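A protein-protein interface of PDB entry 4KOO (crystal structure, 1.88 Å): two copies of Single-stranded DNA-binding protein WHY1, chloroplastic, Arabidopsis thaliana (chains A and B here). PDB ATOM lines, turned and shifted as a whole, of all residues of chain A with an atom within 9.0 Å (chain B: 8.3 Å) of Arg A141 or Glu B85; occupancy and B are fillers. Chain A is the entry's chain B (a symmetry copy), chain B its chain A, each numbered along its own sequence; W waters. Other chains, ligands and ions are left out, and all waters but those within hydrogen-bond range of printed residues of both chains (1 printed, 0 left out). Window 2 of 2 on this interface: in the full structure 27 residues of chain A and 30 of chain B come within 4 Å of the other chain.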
ATOM      1  N   LYS A  17      -6.285  19.445   4.031  1.00  0.00           N
ATOM      2  CA  LYS A  17      -6.116  20.633   4.836  1.00  0.00           C
ATOM      3  C   LYS A  17      -4.736  21.259   4.572  1.00  0.00           C
ATOM      4  O   LYS A  17      -3.969  20.774   3.751  1.00  0.00           O
ATOM      5  CB  LYS A  17      -6.303  20.297   6.325  1.00  0.00           C
ATOM      6  CG  LYS A  17      -7.744  19.817   6.648  1.00  0.00           C
ATOM      7  CD  LYS A  17      -8.757  20.928   6.450  1.00  0.00           C
ATOM      8  CE  LYS A  17     -10.158  20.380   6.620  1.00  0.00           C
ATOM      9  NZ  LYS A  17     -11.203  21.377   6.699  1.00  0.00           N
ATOM     10  N   PRO A  83     -20.696  13.772  21.819  1.00  0.00           N
ATOM     11  CA  PRO A  83     -20.367  14.887  20.923  1.00  0.00           C
ATOM     12  C   PRO A  83     -18.978  15.510  21.180  1.00  0.00           C
ATOM     13  O   PRO A  83     -18.319  15.951  20.241  1.00  0.00           O
ATOM     14  CB  PRO A  83     -21.476  15.905  21.224  1.00  0.00           C
ATOM     15  CG  PRO A  83     -22.579  15.110  21.787  1.00  0.00           C
ATOM     16  CD  PRO A  83     -21.930  14.021  22.582  1.00  0.00           C
ATOM     17  N   LEU A 112     -12.089  19.532  18.844  1.00  0.00           N
ATOM     18  CA  LEU A 112     -11.137  20.627  18.823  1.00  0.00           C
ATOM     19  C   LEU A 112     -11.392  21.517  20.035  1.00  0.00           C
ATOM     20  O   LEU A 112     -12.532  21.679  20.473  1.00  0.00           O
ATOM     21  CB  LEU A 112     -11.292  21.444  17.538  1.00  0.00           C
ATOM     22  CG  LEU A 112     -10.811  20.778  16.242  1.00  0.00           C
ATOM     23  CD1 LEU A 112     -11.177  21.643  15.051  1.00  0.00           C
ATOM     24  CD2 LEU A 112      -9.319  20.563  16.272  1.00  0.00           C
ATOM     25  N   GLY A 115     -13.873  24.536  19.923  1.00  0.00           N
ATOM     26  CA  GLY A 115     -14.415  24.491  18.576  1.00  0.00           C
ATOM     27  C   GLY A 115     -15.385  23.356  18.402  1.00  0.00           C
ATOM     28  O   GLY A 115     -15.466  22.466  19.257  1.00  0.00           O
ATOM     29  N   SER A 116     -16.128  23.384  17.293  1.00  0.00           N
ATOM     30  CA  SER A 116     -17.134  22.383  17.046  1.00  0.00           C
ATOM     31  C   SER A 116     -16.618  21.237  16.164  1.00  0.00           C
ATOM     32  O   SER A 116     -17.320  20.253  15.977  1.00  0.00           O
ATOM     33  CB  SER A 116     -18.378  23.020  16.429  1.00  0.00           C
ATOM     34  OG  SER A 116     -18.127  23.561  15.162  1.00  0.00           O
ATOM     35  N   GLY A 117     -15.427  21.383  15.607  1.00  0.00           N
ATOM     36  CA  GLY A 117     -14.823  20.304  14.830  1.00  0.00           C
ATOM     37  C   GLY A 117     -14.110  19.279  15.702  1.00  0.00           C
ATOM     38  O   GLY A 117     -14.234  19.258  16.929  1.00  0.00           O
ATOM     39  N   HIS A 118     -13.362  18.414  15.050  1.00  0.00           N
ATOM     40  CA  HIS A 118     -12.595  17.360  15.694  1.00  0.00           C
ATOM     41  C   HIS A 118     -11.206  17.343  15.082  1.00  0.00           C
ATOM     42  O   HIS A 118     -10.985  17.939  14.033  1.00  0.00           O
ATOM     43  CB  HIS A 118     -13.215  15.992  15.439  1.00  0.00           C
ATOM     44  CG  HIS A 118     -14.292  15.636  16.403  1.00  0.00           C
ATOM     45  ND1 HIS A 118     -15.522  16.251  16.375  1.00  0.00           N
ATOM     46  CD2 HIS A 118     -14.330  14.751  17.430  1.00  0.00           C
ATOM     47  CE1 HIS A 118     -16.271  15.766  17.358  1.00  0.00           C
ATOM     48  NE2 HIS A 118     -15.573  14.846  18.003  1.00  0.00           N
ATOM     49  N   PHE A 119     -10.268  16.662  15.729  1.00  0.00           N
ATOM     50  CA  PHE A 119      -9.021  16.318  15.052  1.00  0.00           C
ATOM     51  C   PHE A 119      -8.818  14.835  15.049  1.00  0.00           C
ATOM     52  O   PHE A 119      -9.333  14.148  15.925  1.00  0.00           O
ATOM     53  CB  PHE A 119      -7.798  17.044  15.652  1.00  0.00           C
ATOM     54  CG  PHE A 119      -7.380  16.597  17.043  1.00  0.00           C
ATOM     55  CD1 PHE A 119      -6.655  15.420  17.246  1.00  0.00           C
ATOM     56  CD2 PHE A 119      -7.594  17.416  18.135  1.00  0.00           C
ATOM     57  CE1 PHE A 119      -6.241  15.055  18.503  1.00  0.00           C
ATOM     58  CE2 PHE A 119      -7.197  17.051  19.414  1.00  0.00           C
ATOM     59  CZ  PHE A 119      -6.493  15.887  19.603  1.00  0.00           C
ATOM     60  N   PRO A 138      -7.067  18.714  11.507  1.00  0.00           N
ATOM     61  CA  PRO A 138      -8.334  19.204  12.046  1.00  0.00           C
ATOM     62  C   PRO A 138      -9.422  19.091  10.976  1.00  0.00           C
ATOM     63  O   PRO A 138      -9.153  19.364   9.832  1.00  0.00           O
ATOM     64  CB  PRO A 138      -8.026  20.676  12.359  1.00  0.00           C
ATOM     65  CG  PRO A 138      -7.089  21.066  11.245  1.00  0.00           C
ATOM     66  CD  PRO A 138      -6.260  19.814  10.923  1.00  0.00           C
ATOM     67  N   ILE A 139     -10.624  18.721  11.405  1.00  0.00           N
ATOM     68  CA  ILE A 139     -11.778  18.384  10.585  1.00  0.00           C
ATOM     69  C   ILE A 139     -12.904  19.290  11.043  1.00  0.00           C
ATOM     70  O   ILE A 139     -13.083  19.484  12.243  1.00  0.00           O
ATOM     71  CB  ILE A 139     -12.156  16.898  10.980  1.00  0.00           C
ATOM     72  CG1 ILE A 139     -10.963  15.996  10.698  1.00  0.00           C
ATOM     73  CG2 ILE A 139     -13.330  16.346  10.282  1.00  0.00           C
ATOM     74  CD1 ILE A 139     -10.441  16.249   9.343  1.00  0.00           C
ATOM     75  N   THR A 140     -13.694  19.817  10.128  1.00  0.00           N
ATOM     76  CA  THR A 140     -14.859  20.595  10.524  1.00  0.00           C
ATOM     77  C   THR A 140     -16.008  19.701  11.007  1.00  0.00           C
ATOM     78  O   THR A 140     -16.033  18.484  10.792  1.00  0.00           O
ATOM     79  CB  THR A 140     -15.387  21.449   9.384  1.00  0.00           C
ATOM     80  OG1 THR A 140     -15.940  20.583   8.383  1.00  0.00           O
ATOM     81  CG2 THR A 140     -14.293  22.343   8.784  1.00  0.00           C
ATOM     82  N   ARG A 141     -16.943  20.308  11.705  1.00  0.00           N
ATOM     83  CA  ARG A 141     -18.106  19.581  12.151  1.00  0.00           C
ATOM     84  C   ARG A 141     -18.809  18.875  10.974  1.00  0.00           C
ATOM     85  O   ARG A 141     -19.224  17.704  11.078  1.00  0.00           O
ATOM     86  CB  ARG A 141     -19.040  20.589  12.795  1.00  0.00           C
ATOM     87  CG  ARG A 141     -20.318  20.040  13.261  1.00  0.00           C
ATOM     88  CD  ARG A 141     -20.986  21.111  14.065  1.00  0.00           C
ATOM     89  NE  ARG A 141     -22.373  20.781  14.280  1.00  0.00           N
ATOM     90  CZ  ARG A 141     -23.339  21.681  14.391  1.00  0.00           C
ATOM     91  NH1 ARG A 141     -23.046  22.970  14.328  1.00  0.00           N
ATOM     92  NH2 ARG A 141     -24.590  21.276  14.587  1.00  0.00           N
ATOM     93  N   ALA A 142     -18.953  19.584   9.856  1.00  0.00           N
ATOM     94  CA  ALA A 142     -19.628  19.014   8.686  1.00  0.00           C
ATOM     95  C   ALA A 142     -18.808  17.834   8.121  1.00  0.00           C
ATOM     96  O   ALA A 142     -19.384  16.794   7.780  1.00  0.00           O
ATOM     97  CB  ALA A 142     -19.825  20.095   7.584  1.00  0.00           C
ATOM     98  N   GLU A 143     -17.481  17.977   8.080  1.00  0.00           N
ATOM     99  CA  GLU A 143     -16.616  16.922   7.575  1.00  0.00           C
ATOM    100  C   GLU A 143     -16.690  15.687   8.458  1.00  0.00           C
ATOM    101  O   GLU A 143     -16.703  14.555   7.949  1.00  0.00           O
ATOM    102  CB  GLU A 143     -15.160  17.365   7.398  1.00  0.00           C
ATOM    103  CG  GLU A 143     -14.950  18.362   6.302  1.00  0.00           C
ATOM    104  CD  GLU A 143     -13.656  19.178   6.415  1.00  0.00           C
ATOM    105  OE1 GLU A 143     -13.051  19.238   7.490  1.00  0.00           O
ATOM    106  OE2 GLU A 143     -13.230  19.758   5.401  1.00  0.00           O
ATOM    107  N   PHE A 144     -16.752  15.901   9.771  1.00  0.00           N
ATOM    108  CA  PHE A 144     -16.867  14.819  10.744  1.00  0.00           C
ATOM    109  C   PHE A 144     -18.240  14.137  10.594  1.00  0.00           C
ATOM    110  O   PHE A 144     -18.358  12.899  10.703  1.00  0.00           O
ATOM    111  CB  PHE A 144     -16.712  15.379  12.175  1.00  0.00           C
ATOM    112  CG  PHE A 144     -16.532  14.307  13.240  1.00  0.00           C
ATOM    113  CD1 PHE A 144     -15.364  13.566  13.318  1.00  0.00           C
ATOM    114  CD2 PHE A 144     -17.515  14.054  14.137  1.00  0.00           C
ATOM    115  CE1 PHE A 144     -15.225  12.548  14.287  1.00  0.00           C
ATOM    116  CE2 PHE A 144     -17.366  13.077  15.112  1.00  0.00           C
ATOM    117  CZ  PHE A 144     -16.229  12.352  15.188  1.00  0.00           C
ATOM    118  N   ALA A 145     -19.268  14.936  10.343  1.00  0.00           N
ATOM    119  CA  ALA A 145     -20.623  14.387  10.177  1.00  0.00           C
ATOM    120  C   ALA A 145     -20.661  13.476   8.951  1.00  0.00           C
ATOM    121  O   ALA A 145     -21.331  12.443   8.976  1.00  0.00           O
ATOM    122  CB  ALA A 145     -21.710  15.481  10.044  1.00  0.00           C
ATOM    123  N   VAL A 146     -19.964  13.850   7.888  1.00  0.00           N
ATOM    124  CA  VAL A 146     -19.874  12.949   6.722  1.00  0.00           C
ATOM    125  C   VAL A 146     -19.155  11.647   7.079  1.00  0.00           C
ATOM    126  O   VAL A 146     -19.614  10.560   6.716  1.00  0.00           O
ATOM    127  CB  VAL A 146     -19.191  13.629   5.542  1.00  0.00           C
ATOM    128  CG1 VAL A 146     -18.870  12.635   4.421  1.00  0.00           C
ATOM    129  CG2 VAL A 146     -20.045  14.783   5.018  1.00  0.00           C
ATOM    130  N   LEU A 147     -18.022  11.742   7.792  1.00  0.00           N
ATOM    131  CA  LEU A 147     -17.358  10.537   8.264  1.00  0.00           C
ATOM    132  C   LEU A 147     -18.287   9.643   9.057  1.00  0.00           C
ATOM    133  O   LEU A 147     -18.329   8.443   8.809  1.00  0.00           O
ATOM    134  CB  LEU A 147     -16.117  10.833   9.081  1.00  0.00           C
ATOM    135  CG  LEU A 147     -14.961  11.505   8.288  1.00  0.00           C
ATOM    136  CD1 LEU A 147     -13.823  11.763   9.258  1.00  0.00           C
ATOM    137  CD2 LEU A 147     -14.523  10.689   7.073  1.00  0.00           C
ATOM    138  N   ILE A 148     -18.991  10.212  10.028  1.00  0.00           N
ATOM    139  CA  ILE A 148     -19.832   9.411  10.884  1.00  0.00           C
ATOM    140  C   ILE A 148     -20.970   8.761  10.110  1.00  0.00           C
ATOM    141  O   ILE A 148     -21.326   7.594  10.351  1.00  0.00           O
ATOM    142  CB  ILE A 148     -20.339  10.255  12.045  1.00  0.00           C
ATOM    143  CG1 ILE A 148     -19.159  10.704  12.930  1.00  0.00           C
ATOM    144  CG2 ILE A 148     -21.354   9.463  12.897  1.00  0.00           C
ATOM    145  CD1 ILE A 148     -18.427   9.621  13.605  1.00  0.00           C
ATOM    146  N   SER A 149     -21.545   9.503   9.175  1.00  0.00           N
ATOM    147  CA  SER A 149     -22.550   8.952   8.270  1.00  0.00           C
ATOM    148  C   SER A 149     -22.005   7.745   7.473  1.00  0.00           C
ATOM    149  O   SER A 149     -22.640   6.673   7.405  1.00  0.00           O
ATOM    150  CB  SER A 149     -23.020  10.038   7.320  1.00  0.00           C
ATOM    151  OG  SER A 149     -23.841   9.483   6.334  1.00  0.00           O
ATOM    152  N   THR B  73     -20.116  17.767   1.748  1.00  0.00           N
ATOM    153  CA  THR B  73     -19.848  18.473   3.017  1.00  0.00           C
ATOM    154  C   THR B  73     -21.020  19.350   3.467  1.00  0.00           C
ATOM    155  O   THR B  73     -21.343  19.375   4.660  1.00  0.00           O
ATOM    156  CB  THR B  73     -18.501  19.266   2.934  1.00  0.00           C
ATOM    157  OG1 THR B  73     -17.470  18.377   2.479  1.00  0.00           O
ATOM    158  CG2 THR B  73     -18.130  19.804   4.265  1.00  0.00           C
ATOM    159  N   GLY B  76     -23.511  17.279   5.007  1.00  0.00           N
ATOM    160  CA  GLY B  76     -23.032  17.027   6.341  1.00  0.00           C
ATOM    161  C   GLY B  76     -23.464  18.075   7.329  1.00  0.00           C
ATOM    162  O   GLY B  76     -23.887  17.760   8.445  1.00  0.00           O
ATOM    163  N   THR B  77     -23.383  19.345   6.930  1.00  0.00           N
ATOM    164  CA  THR B  77     -23.882  20.419   7.758  1.00  0.00           C
ATOM    165  C   THR B  77     -25.348  20.238   8.054  1.00  0.00           C
ATOM    166  O   THR B  77     -25.773  20.369   9.204  1.00  0.00           O
ATOM    167  CB  THR B  77     -23.676  21.796   7.067  1.00  0.00           C
ATOM    168  OG1 THR B  77     -22.280  22.076   6.958  1.00  0.00           O
ATOM    169  CG2 THR B  77     -24.397  22.893   7.781  1.00  0.00           C
ATOM    170  N   LEU B  78     -26.132  19.949   7.014  1.00  0.00           N
ATOM    171  CA  LEU B  78     -27.579  19.851   7.143  1.00  0.00           C
ATOM    172  C   LEU B  78     -28.011  18.683   8.029  1.00  0.00           C
ATOM    173  O   LEU B  78     -28.910  18.815   8.899  1.00  0.00           O
ATOM    174  CB  LEU B  78     -28.222  19.752   5.745  1.00  0.00           C
ATOM    175  CG  LEU B  78     -28.251  21.058   4.955  1.00  0.00           C
ATOM    176  CD1 LEU B  78     -28.601  20.901   3.486  1.00  0.00           C
ATOM    177  CD2 LEU B  78     -29.215  22.012   5.607  1.00  0.00           C
ATOM    178  N   VAL B  79     -27.381  17.537   7.840  1.00  0.00           N
ATOM    179  CA  VAL B  79     -27.761  16.383   8.644  1.00  0.00           C
ATOM    180  C   VAL B  79     -27.322  16.502  10.131  1.00  0.00           C
ATOM    181  O   VAL B  79     -27.824  15.784  10.982  1.00  0.00           O
ATOM    182  CB  VAL B  79     -27.366  15.057   8.020  1.00  0.00           C
ATOM    183  CG1 VAL B  79     -27.988  14.895   6.637  1.00  0.00           C
ATOM    184  CG2 VAL B  79     -25.857  14.857   7.930  1.00  0.00           C
ATOM    185  N   SER B  80     -26.387  17.374  10.425  1.00  0.00           N
ATOM    186  CA  SER B  80     -25.869  17.477  11.787  1.00  0.00           C
ATOM    187  C   SER B  80     -26.366  18.714  12.511  1.00  0.00           C
ATOM    188  O   SER B  80     -25.932  18.984  13.628  1.00  0.00           O
ATOM    189  CB  SER B  80     -24.330  17.388  11.839  1.00  0.00           C
ATOM    190  OG  SER B  80     -23.692  18.392  11.100  1.00  0.00           O
ATOM    191  N   LEU B  81     -27.273  19.452  11.893  1.00  0.00           N
ATOM    192  CA  LEU B  81     -27.795  20.668  12.508  1.00  0.00           C
ATOM    193  C   LEU B  81     -28.554  20.358  13.783  1.00  0.00           C
ATOM    194  O   LEU B  81     -29.254  19.337  13.893  1.00  0.00           O
ATOM    195  CB  LEU B  81     -28.773  21.377  11.589  1.00  0.00           C
ATOM    196  CG  LEU B  81     -28.328  22.210  10.429  1.00  0.00           C
ATOM    197  CD1 LEU B  81     -29.563  22.656   9.723  1.00  0.00           C
ATOM    198  CD2 LEU B  81     -27.445  23.406  10.851  1.00  0.00           C
ATOM    199  N   GLY B  82     -28.431  21.257  14.745  1.00  0.00           N
ATOM    200  CA  GLY B  82     -29.291  21.224  15.917  1.00  0.00           C
ATOM    201  C   GLY B  82     -30.720  21.447  15.454  1.00  0.00           C
ATOM    202  O   GLY B  82     -30.971  21.954  14.370  1.00  0.00           O
ATOM    203  N   PRO B  83     -31.695  21.075  16.286  1.00  0.00           N
ATOM    204  CA  PRO B  83     -33.098  21.132  15.843  1.00  0.00           C
ATOM    205  C   PRO B  83     -33.606  22.506  15.378  1.00  0.00           C
ATOM    206  O   PRO B  83     -34.493  22.556  14.503  1.00  0.00           O
ATOM    207  CB  PRO B  83     -33.865  20.634  17.076  1.00  0.00           C
ATOM    208  CG  PRO B  83     -32.900  19.706  17.753  1.00  0.00           C
ATOM    209  CD  PRO B  83     -31.543  20.371  17.569  1.00  0.00           C
ATOM    210  N   ARG B  84     -33.053  23.592  15.927  1.00  0.00           N
ATOM    211  CA  ARG B  84     -33.423  24.940  15.501  1.00  0.00           C
ATOM    212  C   ARG B  84     -32.183  25.765  15.202  1.00  0.00           C
ATOM    213  O   ARG B  84     -32.176  27.002  15.347  1.00  0.00           O
ATOM    214  CB  ARG B  84     -34.261  25.653  16.567  1.00  0.00           C
ATOM    215  CG  ARG B  84     -35.705  25.128  16.678  1.00  0.00           C
ATOM    216  CD  ARG B  84     -36.542  26.100  17.513  1.00  0.00           C
ATOM    217  NE  ARG B  84     -37.519  26.904  16.752  1.00  0.00           N
ATOM    218  CZ  ARG B  84     -37.330  28.138  16.265  1.00  0.00           C
ATOM    219  NH1 ARG B  84     -38.327  28.726  15.630  1.00  0.00           N
ATOM    220  NH2 ARG B  84     -36.168  28.798  16.381  1.00  0.00           N
ATOM    221  N   GLU B  85     -31.138  25.083  14.760  1.00  0.00           N
ATOM    222  CA  GLU B  85     -29.932  25.750  14.307  1.00  0.00           C
ATOM    223  C   GLU B  85     -30.058  26.295  12.879  1.00  0.00           C
ATOM    224  O   GLU B  85     -30.588  25.628  11.998  1.00  0.00           O
ATOM    225  CB  GLU B  85     -28.737  24.775  14.408  1.00  0.00           C
ATOM    226  CG  GLU B  85     -27.386  25.405  14.112  1.00  0.00           C
ATOM    227  CD  GLU B  85     -26.238  24.473  14.294  1.00  0.00           C
ATOM    228  OE1 GLU B  85     -26.497  23.298  14.631  1.00  0.00           O
ATOM    229  OE2 GLU B  85     -25.065  24.894  14.044  1.00  0.00           O
ATOM    230  N   SER B  86     -29.524  27.489  12.646  1.00  0.00           N
ATOM    231  CA  SER B  86     -29.490  28.063  11.309  1.00  0.00           C
ATOM    232  C   SER B  86     -28.211  27.703  10.566  1.00  0.00           C
ATOM    233  O   SER B  86     -27.185  27.374  11.167  1.00  0.00           O
ATOM    234  CB  SER B  86     -29.629  29.585  11.387  1.00  0.00           C
ATOM    235  OG  SER B  86     -30.849  29.929  12.036  1.00  0.00           O
ATOM    236  N   CYS B  87     -28.278  27.732   9.248  1.00  0.00           N
ATOM    237  CA  CYS B  87     -27.059  27.610   8.465  1.00  0.00           C
ATOM    238  C   CYS B  87     -27.186  28.417   7.176  1.00  0.00           C
ATOM    239  O   CYS B  87     -28.275  28.828   6.756  1.00  0.00           O
ATOM    240  CB  CYS B  87     -26.647  26.163   8.198  1.00  0.00           C
ATOM    241  SG  CYS B  87     -27.730  25.169   7.189  1.00  0.00           S
ATOM    242  N   GLU B  88     -26.040  28.657   6.579  1.00  0.00           N
ATOM    243  CA  GLU B  88     -25.962  29.515   5.424  1.00  0.00           C
ATOM    244  C   GLU B  88     -24.770  29.056   4.595  1.00  0.00           C
ATOM    245  O   GLU B  88     -23.715  28.746   5.171  1.00  0.00           O
ATOM    246  CB  GLU B  88     -25.779  30.938   5.925  1.00  0.00           C
ATOM    247  CG  GLU B  88     -25.900  31.983   4.870  1.00  0.00           C
ATOM    248  CD  GLU B  88     -25.899  33.376   5.472  1.00  0.00           C
ATOM    249  OE1 GLU B  88     -25.249  33.575   6.531  1.00  0.00           O
ATOM    250  OE2 GLU B  88     -26.565  34.242   4.887  1.00  0.00           O
ATOM    251  N   VAL B 109     -30.868  28.277   5.335  1.00  0.00           N
ATOM    252  CA  VAL B 109     -31.783  27.262   5.848  1.00  0.00           C
ATOM    253  C   VAL B 109     -31.945  27.574   7.332  1.00  0.00           C
ATOM    254  O   VAL B 109     -30.980  27.565   8.081  1.00  0.00           O
ATOM    255  CB  VAL B 109     -31.252  25.826   5.658  1.00  0.00           C
ATOM    256  CG1 VAL B 109     -32.221  24.832   6.217  1.00  0.00           C
ATOM    257  CG2 VAL B 109     -31.016  25.509   4.183  1.00  0.00           C
ATOM    258  N   GLU B 110     -33.164  27.889   7.756  1.00  0.00           N
ATOM    259  CA  GLU B 110     -33.386  28.329   9.130  1.00  0.00           C
ATOM    260  C   GLU B 110     -34.748  27.881   9.599  1.00  0.00           C
ATOM    261  O   GLU B 110     -35.659  27.729   8.796  1.00  0.00           O
ATOM    262  CB  GLU B 110     -33.366  29.853   9.231  1.00  0.00           C
ATOM    263  CG  GLU B 110     -32.082  30.467   8.745  1.00  0.00           C
ATOM    264  CD  GLU B 110     -32.022  31.963   8.957  1.00  0.00           C
ATOM    265  OE1 GLU B 110     -32.864  32.512   9.706  1.00  0.00           O
ATOM    266  OE2 GLU B 110     -31.112  32.583   8.365  1.00  0.00           O
ATOM    267  N   PRO B 111     -34.898  27.732  10.914  1.00  0.00           N
ATOM    268  CA  PRO B 111     -36.230  27.462  11.462  1.00  0.00           C
ATOM    269  C   PRO B 111     -37.157  28.632  11.206  1.00  0.00           C
ATOM    270  O   PRO B 111     -36.733  29.782  11.110  1.00  0.00           O
ATOM    271  CB  PRO B 111     -35.973  27.268  12.966  1.00  0.00           C
ATOM    272  CG  PRO B 111     -34.698  27.915  13.258  1.00  0.00           C
ATOM    273  CD  PRO B 111     -33.868  27.807  11.973  1.00  0.00           C
ATOM    274  N   HIS B 118     -39.278  24.998   8.664  1.00  0.00           N
ATOM    275  CA  HIS B 118     -38.034  25.656   8.258  1.00  0.00           C
ATOM    276  C   HIS B 118     -38.366  26.426   7.009  1.00  0.00           C
ATOM    277  O   HIS B 118     -39.421  26.226   6.412  1.00  0.00           O
ATOM    278  CB  HIS B 118     -36.937  24.640   7.919  1.00  0.00           C
ATOM    279  CG  HIS B 118     -36.169  24.140   9.097  1.00  0.00           C
ATOM    280  ND1 HIS B 118     -36.710  23.286  10.027  1.00  0.00           N
ATOM    281  CD2 HIS B 118     -34.915  24.425   9.536  1.00  0.00           C
ATOM    282  CE1 HIS B 118     -35.815  23.029  10.969  1.00  0.00           C
ATOM    283  NE2 HIS B 118     -34.715  23.708  10.695  1.00  0.00           N
ATOM    284  N   PHE B 144     -39.458  18.539   6.034  1.00  0.00           N
ATOM    285  CA  PHE B 144     -38.046  18.661   6.380  1.00  0.00           C
ATOM    286  C   PHE B 144     -37.504  17.320   6.812  1.00  0.00           C
ATOM    287  O   PHE B 144     -36.360  16.954   6.477  1.00  0.00           O
ATOM    288  CB  PHE B 144     -37.881  19.704   7.490  1.00  0.00           C
ATOM    289  CG  PHE B 144     -36.466  20.145   7.704  1.00  0.00           C
ATOM    290  CD1 PHE B 144     -35.855  21.005   6.802  1.00  0.00           C
ATOM    291  CD2 PHE B 144     -35.747  19.702   8.786  1.00  0.00           C
ATOM    292  CE1 PHE B 144     -34.532  21.390   6.983  1.00  0.00           C
ATOM    293  CE2 PHE B 144     -34.408  20.101   8.975  1.00  0.00           C
ATOM    294  CZ  PHE B 144     -33.828  20.943   8.093  1.00  0.00           C
HETATM  295  O   HOH W   1     -24.179  21.225  11.279  1.00  0.00           O
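O of Ser B80 sits at hydrogen-bond distance from NH2 of Arg A141, at 2.8 Å. The side-chain carboxylate (OE1) of Glu B85 is in salt-bridge range of the guanidinium group (NH2) of Arg A141, 2.8 Å away.
The backbone carbonyl oxygen (O) of Thr B77 lies within hydrogen-bond range of the side-chain hydroxyl (OG) of Ser B80. The backbone carbonyl oxygen of Gly B76 sits at hydrogen-bond distance from the side-chain hydroxyl of Ser B80. OG1 of Thr A140 sits close to N of Ala A142 (3.5 Å). N of Gly B82 lies within hydrogen-bond range of OE1 of Glu B85 (2.8 Å).
Among the printed residues, pairs that only touch across the chains: Arg A141 with Leu B81, Arg A141 with Gly B82, Ala A142 with Thr B73, Ala A142 with Gly B76, Ala A142 with Thr B77, Ala A145 with Gly B76, Ala A145 with Ser B80 and Val A146 with Gly B76.
Of chain A, only Arg A141 comes within 4 Å of Glu B85. Ala A142 touches three residues of chain B. Of chain A, only Arg A141 comes within 4 Å of Leu B81. Gly B82 touches one residue of chain A. Of the printed residues of chain A, Thr B73 touches Ala A142. Of the printed residues of chain B, Ala A145 touches Gly B76 (3.5 Å) and Ser B80 (3.7 Å). Printed residues of chain A within 4 Å of Thr B77: Ala A142. Printed residues of chain A within 4 Å of Ser B80: Arg A141 (2.8 Å) and Ala A145 (3.7 Å). The nearest residue of chain B that does not touch Arg A141 is Gly B76 (5.4 Å). The nearest residue of chain A that does not touch Glu B85 is Ser A116 (7.2 Å). The nearest printed residue of chain A that does not touch Thr B73 is Glu A143 (4.04 Å).
Hydrophobic or aromatic side chains of chain A within 4 Å of the printed part of chain B: Ala A142, Ala A145 and Val A146. Of the 19 printed residues of chain B, 7 touch a printed residue of chain A. Among the printed residues, 10 pairs touch across the chains. Among the printed residues, Asp or Glu carboxylates within 4 Å of a Lys or Arg side-chain nitrogen of the other chain: Arg A141 with Glu B85.
3 positions are printed for both chains.
Water W1 lies within hydrogen-bond range of O of Thr B77 (2.8 Å), OG of Ser B80 (2.9 Å) and NH2 of Arg A141 (3.3 Å).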
